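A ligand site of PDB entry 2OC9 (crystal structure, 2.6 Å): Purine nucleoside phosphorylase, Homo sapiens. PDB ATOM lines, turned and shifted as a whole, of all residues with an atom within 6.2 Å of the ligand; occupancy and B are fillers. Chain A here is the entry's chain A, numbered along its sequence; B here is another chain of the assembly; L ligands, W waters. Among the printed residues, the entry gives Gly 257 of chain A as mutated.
Merely in contact with the ligand: His 86 (3.9 Å), Ala 116 (3.4 Å), Ala 117 (3.8 Å), Gly 118 (3.6 Å), Phe 200 (3.5 Å), Val 217 (3.5 Å), Gly 218 (3.5 Å), Thr 242 (3.8 Å), Val 245 (3.6 Å), Val 260 (3.4 Å) and Phe 159 of chain B (3.6 Å). 15 residues have an atom within 4 Å of the ligand: His 86, Tyr 88, Ala 116, Ala 117, Gly 118, Phe 200, Glu 201, Val 217, Gly 218, Met 219, Thr 242, Asn 243, Val 245, Val 260 and Phe 159 of chain B. Along chain A the residues within 4 Å of the ligand span positions 86 to 260.
The side-chain amide oxygen of Asn 243 lies within hydrogen-bond range of the side-chain hydroxyl of Thr 242 (2.7 Å). The backbone carbonyl oxygen of Asn 243 is in hydrogen-bond range of the backbone NH of Gly 119 (2.8 Å). The backbone NH of Met 219 sits at hydrogen-bond distance from the side-chain hydroxyl of Tyr 192 (3.4 Å). The side-chain hydroxyl (OH) of Tyr 88 lies within hydrogen-bond range of a ring nitrogen (ND1) of His 86 (3.3 Å). The backbone NH of Val 195 sits at hydrogen-bond distance from the backbone carbonyl oxygen of Gly 218 (3.0 Å). The backbone carbonyl oxygen (O) of Gly 118 is in hydrogen-bond range of the backbone NH (N) of Val 217, 2.9 Å away. N of Val 245 sits at hydrogen-bond distance from O of Gly 119 (3.0 Å). The backbone NH (N) of Thr 242 is in hydrogen-bond range of the backbone carbonyl oxygen (O) of Ala 117, at 3.1 Å.
The side-chain carboxylate of Glu 201 sits at hydrogen-bond distance from a nitrogen (N3) of the ligand, at 2.8 Å. OD1 of Asn 243 lies within hydrogen-bond range of N2 of the ligand, at 2.8 Å. The backbone NH (N) of Met 219 is in hydrogen-bond range of an oxygen (O3) of the ligand, 3.1 Å away. OH of Tyr 88 lies within hydrogen-bond range of O2 of the ligand (3.2 Å).
Water W1 bridges OE1 of Glu 201 (2.6 Å) and O4 of the ligand (2.7 Å).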
ATOM      1  N   HIS A  86     -22.857 -16.494 -15.845  1.00  0.00           N
ATOM      2  CA  HIS A  86     -22.582 -17.903 -15.872  1.00  0.00           C
ATOM      3  C   HIS A  86     -23.749 -18.624 -15.291  1.00  0.00           C
ATOM      4  O   HIS A  86     -24.387 -18.169 -14.325  1.00  0.00           O
ATOM      5  CB  HIS A  86     -21.361 -18.271 -15.051  1.00  0.00           C
ATOM      6  CG  HIS A  86     -20.106 -17.540 -15.423  1.00  0.00           C
ATOM      7  ND1 HIS A  86     -19.810 -16.280 -14.943  1.00  0.00           N
ATOM      8  CD2 HIS A  86     -19.051 -17.898 -16.200  1.00  0.00           C
ATOM      9  CE1 HIS A  86     -18.643 -15.897 -15.408  1.00  0.00           C
ATOM     10  NE2 HIS A  86     -18.163 -16.859 -16.171  1.00  0.00           N
ATOM     11  N   TYR A  88     -23.367 -21.183 -13.555  1.00  0.00           N
ATOM     12  CA  TYR A  88     -23.116 -21.544 -12.177  1.00  0.00           C
ATOM     13  C   TYR A  88     -23.495 -20.461 -11.228  1.00  0.00           C
ATOM     14  O   TYR A  88     -23.628 -20.763 -10.094  1.00  0.00           O
ATOM     15  CB  TYR A  88     -21.695 -22.060 -11.912  1.00  0.00           C
ATOM     16  CG  TYR A  88     -20.649 -21.039 -12.184  1.00  0.00           C
ATOM     17  CD1 TYR A  88     -20.390 -20.013 -11.258  1.00  0.00           C
ATOM     18  CD2 TYR A  88     -19.908 -21.078 -13.384  1.00  0.00           C
ATOM     19  CE1 TYR A  88     -19.450 -19.005 -11.542  1.00  0.00           C
ATOM     20  CE2 TYR A  88     -18.971 -20.149 -13.651  1.00  0.00           C
ATOM     21  CZ  TYR A  88     -18.742 -19.103 -12.733  1.00  0.00           C
ATOM     22  OH  TYR A  88     -17.804 -18.149 -13.037  1.00  0.00           O
ATOM     23  N   ASN A 115     -12.086 -17.153 -23.240  1.00  0.00           N
ATOM     24  CA  ASN A 115     -12.449 -17.705 -21.941  1.00  0.00           C
ATOM     25  C   ASN A 115     -11.190 -18.350 -21.432  1.00  0.00           C
ATOM     26  O   ASN A 115     -10.229 -18.394 -22.149  1.00  0.00           O
ATOM     27  CB  ASN A 115     -13.637 -18.729 -22.080  1.00  0.00           C
ATOM     28  CG  ASN A 115     -13.276 -19.971 -22.918  1.00  0.00           C
ATOM     29  OD1 ASN A 115     -12.233 -20.554 -22.722  1.00  0.00           O
ATOM     30  ND2 ASN A 115     -14.141 -20.370 -23.836  1.00  0.00           N
ATOM     31  N   ALA A 116     -11.198 -18.821 -20.200  1.00  0.00           N
ATOM     32  CA  ALA A 116     -10.072 -19.532 -19.592  1.00  0.00           C
ATOM     33  C   ALA A 116     -10.540 -20.966 -19.502  1.00  0.00           C
ATOM     34  O   ALA A 116     -11.716 -21.177 -19.363  1.00  0.00           O
ATOM     35  CB  ALA A 116      -9.815 -19.001 -18.192  1.00  0.00           C
ATOM     36  N   ALA A 117      -9.663 -21.951 -19.574  1.00  0.00           N
ATOM     37  CA  ALA A 117     -10.129 -23.326 -19.670  1.00  0.00           C
ATOM     38  C   ALA A 117      -8.985 -24.220 -19.279  1.00  0.00           C
ATOM     39  O   ALA A 117      -7.827 -23.805 -19.333  1.00  0.00           O
ATOM     40  CB  ALA A 117     -10.578 -23.602 -21.042  1.00  0.00           C
ATOM     41  N   GLY A 118      -9.312 -25.412 -18.815  1.00  0.00           N
ATOM     42  CA  GLY A 118      -8.303 -26.349 -18.386  1.00  0.00           C
ATOM     43  C   GLY A 118      -7.975 -27.155 -19.619  1.00  0.00           C
ATOM     44  O   GLY A 118      -8.859 -27.413 -20.485  1.00  0.00           O
ATOM     45  N   GLY A 119      -6.685 -27.522 -19.731  1.00  0.00           N
ATOM     46  CA  GLY A 119      -6.207 -28.242 -20.865  1.00  0.00           C
ATOM     47  C   GLY A 119      -6.524 -29.666 -20.581  1.00  0.00           C
ATOM     48  O   GLY A 119      -6.281 -30.155 -19.469  1.00  0.00           O
ATOM     49  N   TYR A 192     -13.661 -27.306 -27.521  1.00  0.00           N
ATOM     50  CA  TYR A 192     -13.937 -26.815 -26.144  1.00  0.00           C
ATOM     51  C   TYR A 192     -15.217 -27.530 -25.588  1.00  0.00           C
ATOM     52  O   TYR A 192     -16.276 -27.537 -26.260  1.00  0.00           O
ATOM     53  CB  TYR A 192     -14.194 -25.318 -26.219  1.00  0.00           C
ATOM     54  CG  TYR A 192     -14.661 -24.689 -24.952  1.00  0.00           C
ATOM     55  CD1 TYR A 192     -13.734 -24.118 -24.066  1.00  0.00           C
ATOM     56  CD2 TYR A 192     -16.035 -24.634 -24.632  1.00  0.00           C
ATOM     57  CE1 TYR A 192     -14.128 -23.527 -22.894  1.00  0.00           C
ATOM     58  CE2 TYR A 192     -16.459 -24.022 -23.468  1.00  0.00           C
ATOM     59  CZ  TYR A 192     -15.484 -23.464 -22.606  1.00  0.00           C
ATOM     60  OH  TYR A 192     -15.832 -22.834 -21.461  1.00  0.00           O
ATOM     61  N   VAL A 195     -18.965 -27.570 -19.306  1.00  0.00           N
ATOM     62  CA  VAL A 195     -19.573 -28.178 -18.142  1.00  0.00           C
ATOM     63  C   VAL A 195     -20.055 -27.017 -17.238  1.00  0.00           C
ATOM     64  O   VAL A 195     -19.604 -25.874 -17.338  1.00  0.00           O
ATOM     65  CB  VAL A 195     -18.580 -29.085 -17.362  1.00  0.00           C
ATOM     66  CG1 VAL A 195     -17.969 -30.163 -18.272  1.00  0.00           C
ATOM     67  CG2 VAL A 195     -17.538 -28.257 -16.722  1.00  0.00           C
ATOM     68  N   PRO A 198     -20.028 -24.917 -10.502  1.00  0.00           N
ATOM     69  CA  PRO A 198     -18.815 -24.165 -10.304  1.00  0.00           C
ATOM     70  C   PRO A 198     -17.672 -24.961  -9.711  1.00  0.00           C
ATOM     71  O   PRO A 198     -16.580 -24.427  -9.663  1.00  0.00           O
ATOM     72  CB  PRO A 198     -19.233 -23.179  -9.274  1.00  0.00           C
ATOM     73  CG  PRO A 198     -20.144 -23.927  -8.414  1.00  0.00           C
ATOM     74  CD  PRO A 198     -20.945 -24.745  -9.356  1.00  0.00           C
ATOM     75  N   SER A 199     -17.865 -26.195  -9.256  1.00  0.00           N
ATOM     76  CA  SER A 199     -16.754 -27.020  -8.775  1.00  0.00           C
ATOM     77  C   SER A 199     -15.933 -27.627  -9.922  1.00  0.00           C
ATOM     78  O   SER A 199     -16.455 -27.742 -11.035  1.00  0.00           O
ATOM     79  CB  SER A 199     -17.297 -28.119  -7.875  1.00  0.00           C
ATOM     80  OG  SER A 199     -18.016 -29.061  -8.613  1.00  0.00           O
ATOM     81  N   PHE A 200     -14.670 -28.024  -9.682  1.00  0.00           N
ATOM     82  CA  PHE A 200     -13.766 -28.446 -10.744  1.00  0.00           C
ATOM     83  C   PHE A 200     -13.877 -29.935 -10.883  1.00  0.00           C
ATOM     84  O   PHE A 200     -14.397 -30.575  -9.994  1.00  0.00           O
ATOM     85  CB  PHE A 200     -12.274 -28.080 -10.429  1.00  0.00           C
ATOM     86  CG  PHE A 200     -11.906 -26.636 -10.655  1.00  0.00           C
ATOM     87  CD1 PHE A 200     -11.999 -26.052 -11.905  1.00  0.00           C
ATOM     88  CD2 PHE A 200     -11.402 -25.885  -9.592  1.00  0.00           C
ATOM     89  CE1 PHE A 200     -11.613 -24.702 -12.157  1.00  0.00           C
ATOM     90  CE2 PHE A 200     -10.997 -24.501  -9.788  1.00  0.00           C
ATOM     91  CZ  PHE A 200     -11.118 -23.919 -11.110  1.00  0.00           C
ATOM     92  N   GLU A 201     -13.323 -30.494 -11.933  1.00  0.00           N
ATOM     93  CA  GLU A 201     -13.601 -31.857 -12.325  1.00  0.00           C
ATOM     94  C   GLU A 201     -12.814 -32.809 -11.430  1.00  0.00           C
ATOM     95  O   GLU A 201     -11.745 -32.463 -11.008  1.00  0.00           O
ATOM     96  CB  GLU A 201     -13.138 -32.082 -13.766  1.00  0.00           C
ATOM     97  CG  GLU A 201     -13.934 -31.352 -14.840  1.00  0.00           C
ATOM     98  CD  GLU A 201     -13.731 -29.816 -14.813  1.00  0.00           C
ATOM     99  OE1 GLU A 201     -12.565 -29.323 -14.652  1.00  0.00           O
ATOM    100  OE2 GLU A 201     -14.761 -29.094 -14.902  1.00  0.00           O
ATOM    101  N   VAL A 217     -11.616 -27.466 -21.314  1.00  0.00           N
ATOM    102  CA  VAL A 217     -12.859 -27.476 -20.521  1.00  0.00           C
ATOM    103  C   VAL A 217     -13.091 -26.176 -19.777  1.00  0.00           C
ATOM    104  O   VAL A 217     -12.184 -25.683 -19.081  1.00  0.00           O
ATOM    105  CB  VAL A 217     -12.921 -28.627 -19.520  1.00  0.00           C
ATOM    106  CG1 VAL A 217     -11.825 -28.482 -18.445  1.00  0.00           C
ATOM    107  CG2 VAL A 217     -14.313 -28.685 -18.883  1.00  0.00           C
ATOM    108  N   GLY A 218     -14.285 -25.590 -19.936  1.00  0.00           N
ATOM    109  CA  GLY A 218     -14.688 -24.489 -19.082  1.00  0.00           C
ATOM    110  C   GLY A 218     -16.189 -24.466 -18.830  1.00  0.00           C
ATOM    111  O   GLY A 218     -16.941 -25.391 -19.227  1.00  0.00           O
ATOM    112  N   MET A 219     -16.609 -23.369 -18.223  1.00  0.00           N
ATOM    113  CA  MET A 219     -17.926 -23.194 -17.690  1.00  0.00           C
ATOM    114  C   MET A 219     -18.704 -22.138 -18.406  1.00  0.00           C
ATOM    115  O   MET A 219     -19.766 -21.720 -17.908  1.00  0.00           O
ATOM    116  CB  MET A 219     -17.789 -22.833 -16.234  1.00  0.00           C
ATOM    117  CG  MET A 219     -17.007 -23.881 -15.523  1.00  0.00           C
ATOM    118  SD  MET A 219     -16.859 -23.506 -13.793  1.00  0.00           S
ATOM    119  CE  MET A 219     -15.742 -24.773 -13.277  1.00  0.00           C
ATOM    120  N   SER A 220     -18.234 -21.722 -19.589  1.00  0.00           N
ATOM    121  CA  SER A 220     -18.916 -20.638 -20.333  1.00  0.00           C
ATOM    122  C   SER A 220     -18.911 -20.763 -21.884  1.00  0.00           C
ATOM    123  O   SER A 220     -18.578 -21.786 -22.427  1.00  0.00           O
ATOM    124  CB  SER A 220     -18.219 -19.330 -19.990  1.00  0.00           C
ATOM    125  OG  SER A 220     -16.932 -19.264 -20.593  1.00  0.00           O
ATOM    126  N   THR A 242      -5.335 -22.083 -18.782  1.00  0.00           N
ATOM    127  CA  THR A 242      -4.763 -21.584 -17.568  1.00  0.00           C
ATOM    128  C   THR A 242      -4.270 -22.671 -16.642  1.00  0.00           C
ATOM    129  O   THR A 242      -3.721 -22.368 -15.617  1.00  0.00           O
ATOM    130  CB  THR A 242      -5.786 -20.791 -16.776  1.00  0.00           C
ATOM    131  OG1 THR A 242      -6.961 -21.586 -16.619  1.00  0.00           O
ATOM    132  CG2 THR A 242      -6.142 -19.499 -17.507  1.00  0.00           C
ATOM    133  N   ASN A 243      -4.518 -23.928 -16.945  1.00  0.00           N
ATOM    134  CA  ASN A 243      -4.235 -25.029 -16.006  1.00  0.00           C
ATOM    135  C   ASN A 243      -4.313 -26.308 -16.785  1.00  0.00           C
ATOM    136  O   ASN A 243      -5.100 -26.389 -17.729  1.00  0.00           O
ATOM    137  CB  ASN A 243      -5.187 -25.047 -14.779  1.00  0.00           C
ATOM    138  CG  ASN A 243      -6.721 -25.076 -15.130  1.00  0.00           C
ATOM    139  OD1 ASN A 243      -7.331 -24.075 -15.550  1.00  0.00           O
ATOM    140  ND2 ASN A 243      -7.349 -26.207 -14.875  1.00  0.00           N
ATOM    141  N   VAL A 245      -5.434 -30.048 -16.639  1.00  0.00           N
ATOM    142  CA  VAL A 245      -6.377 -30.623 -15.672  1.00  0.00           C
ATOM    143  C   VAL A 245      -5.743 -31.918 -15.187  1.00  0.00           C
ATOM    144  O   VAL A 245      -5.132 -32.657 -15.963  1.00  0.00           O
ATOM    145  CB  VAL A 245      -7.836 -30.782 -16.170  1.00  0.00           C
ATOM    146  CG1 VAL A 245      -8.323 -29.548 -16.862  1.00  0.00           C
ATOM    147  CG2 VAL A 245      -7.941 -31.922 -17.083  1.00  0.00           C
ATOM    148  N   ALA A 255      -6.289 -27.765  -9.165  1.00  0.00           N
ATOM    149  CA  ALA A 255      -6.914 -26.599  -9.836  1.00  0.00           C
ATOM    150  C   ALA A 255      -7.557 -25.677  -8.818  1.00  0.00           C
ATOM    151  O   ALA A 255      -8.272 -26.116  -7.920  1.00  0.00           O
ATOM    152  CB  ALA A 255      -7.955 -27.055 -10.867  1.00  0.00           C
ATOM    153  N   ASN A 256      -7.266 -24.390  -8.963  1.00  0.00           N
ATOM    154  CA  ASN A 256      -7.797 -23.338  -8.075  1.00  0.00           C
ATOM    155  C   ASN A 256      -8.181 -22.098  -8.874  1.00  0.00           C
ATOM    156  O   ASN A 256      -7.711 -21.910 -10.007  1.00  0.00           O
ATOM    157  CB  ASN A 256      -6.822 -23.020  -6.896  1.00  0.00           C
ATOM    158  CG  ASN A 256      -5.336 -23.009  -7.325  1.00  0.00           C
ATOM    159  OD1 ASN A 256      -4.873 -22.120  -8.041  1.00  0.00           O
ATOM    160  ND2 ASN A 256      -4.578 -23.987  -6.838  1.00  0.00           N
ATOM    161  N   GLY A 257      -9.074 -21.277  -8.304  1.00  0.00           N
ATOM    162  CA  GLY A 257      -9.540 -20.045  -8.931  1.00  0.00           C
ATOM    163  C   GLY A 257      -8.411 -19.030  -8.929  1.00  0.00           C
ATOM    164  O   GLY A 257      -8.448 -18.042  -9.675  1.00  0.00           O
ATOM    165  N   GLU A 258      -7.398 -19.303  -8.107  1.00  0.00           N
ATOM    166  CA  GLU A 258      -6.233 -18.450  -7.944  1.00  0.00           C
ATOM    167  C   GLU A 258      -5.284 -18.541  -9.159  1.00  0.00           C
ATOM    168  O   GLU A 258      -4.916 -17.512  -9.727  1.00  0.00           O
ATOM    169  CB  GLU A 258      -5.480 -18.774  -6.638  1.00  0.00           C
ATOM    170  CG  GLU A 258      -6.277 -19.609  -5.574  1.00  0.00           C
ATOM    171  CD  GLU A 258      -7.375 -18.825  -4.822  1.00  0.00           C
ATOM    172  OE1 GLU A 258      -7.340 -18.821  -3.569  1.00  0.00           O
ATOM    173  OE2 GLU A 258      -8.251 -18.212  -5.480  1.00  0.00           O
ATOM    174  N   VAL A 260      -6.036 -19.742 -12.184  1.00  0.00           N
ATOM    175  CA  VAL A 260      -6.821 -19.299 -13.350  1.00  0.00           C
ATOM    176  C   VAL A 260      -6.723 -17.772 -13.488  1.00  0.00           C
ATOM    177  O   VAL A 260      -6.403 -17.263 -14.569  1.00  0.00           O
ATOM    178  CB  VAL A 260      -8.319 -19.785 -13.314  1.00  0.00           C
ATOM    179  CG1 VAL A 260      -9.068 -19.335 -14.556  1.00  0.00           C
ATOM    180  CG2 VAL A 260      -8.404 -21.307 -13.161  1.00  0.00           C
ATOM    181  N   LEU A 261      -6.993 -17.062 -12.384  1.00  0.00           N
ATOM    182  CA  LEU A 261      -6.913 -15.590 -12.322  1.00  0.00           C
ATOM    183  C   LEU A 261      -5.487 -15.071 -12.553  1.00  0.00           C
ATOM    184  O   LEU A 261      -5.237 -14.276 -13.489  1.00  0.00           O
ATOM    185  CB  LEU A 261      -7.419 -15.078 -10.968  1.00  0.00           C
ATOM    186  CG  LEU A 261      -8.930 -14.854 -10.790  1.00  0.00           C
ATOM    187  CD1 LEU A 261      -9.316 -14.824  -9.296  1.00  0.00           C
ATOM    188  CD2 LEU A 261      -9.420 -13.590 -11.531  1.00  0.00           C
ATOM    189  N   PHE B 159     -15.032 -21.899  -6.405  1.00  0.00           N
ATOM    190  CA  PHE B 159     -14.597 -22.971  -7.325  1.00  0.00           C
ATOM    191  C   PHE B 159     -13.832 -24.070  -6.567  1.00  0.00           C
ATOM    192  O   PHE B 159     -12.634 -24.280  -6.775  1.00  0.00           O
ATOM    193  CB  PHE B 159     -13.726 -22.406  -8.473  1.00  0.00           C
ATOM    194  CG  PHE B 159     -14.402 -21.273  -9.308  1.00  0.00           C
ATOM    195  CD1 PHE B 159     -15.487 -21.518 -10.137  1.00  0.00           C
ATOM    196  CD2 PHE B 159     -13.902 -19.975  -9.312  1.00  0.00           C
ATOM    197  CE1 PHE B 159     -16.080 -20.454 -10.926  1.00  0.00           C
ATOM    198  CE2 PHE B 159     -14.483 -18.927 -10.078  1.00  0.00           C
ATOM    199  CZ  PHE B 159     -15.582 -19.173 -10.881  1.00  0.00           C
HETATM  200  O1  LIG L   1     -11.535 -20.389 -12.385  1.00  0.00           O
HETATM  201  C1  LIG L   1     -12.879 -20.689 -12.772  1.00  0.00           C
HETATM  202  C2  LIG L   1     -13.204 -19.995 -14.087  1.00  0.00           C
HETATM  203  N1  LIG L   1     -12.267 -20.359 -15.157  1.00  0.00           N
HETATM  204  C3  LIG L   1     -14.579 -20.431 -14.620  1.00  0.00           C
HETATM  205  O2  LIG L   1     -15.397 -19.229 -14.827  1.00  0.00           O
HETATM  206  C4  LIG L   1     -14.314 -21.334 -15.861  1.00  0.00           C
HETATM  207  O3  LIG L   1     -15.081 -20.989 -17.023  1.00  0.00           O
HETATM  208  C5  LIG L   1     -12.785 -21.305 -16.170  1.00  0.00           C
HETATM  209  C6  LIG L   1     -11.966 -22.554 -15.989  1.00  0.00           C
HETATM  210  C7  LIG L   1     -10.576 -22.465 -15.876  1.00  0.00           C
HETATM  211  N2  LIG L   1     -10.101 -23.738 -15.671  1.00  0.00           N
HETATM  212  C8  LIG L   1     -11.102 -24.666 -15.638  1.00  0.00           C
HETATM  213  C9  LIG L   1     -11.209 -26.123 -15.446  1.00  0.00           C
HETATM  214  O4  LIG L   1     -10.097 -26.872 -15.254  1.00  0.00           O
HETATM  215  N3  LIG L   1     -12.431 -26.685 -15.450  1.00  0.00           N
HETATM  216  C10 LIG L   1     -13.562 -25.977 -15.638  1.00  0.00           C
HETATM  217  N4  LIG L   1     -13.544 -24.644 -15.818  1.00  0.00           N
HETATM  218  C11 LIG L   1     -12.373 -23.971 -15.821  1.00  0.00           C
HETATM  219  O   HOH W   1     -10.191 -29.047 -13.669  1.00  0.00           O
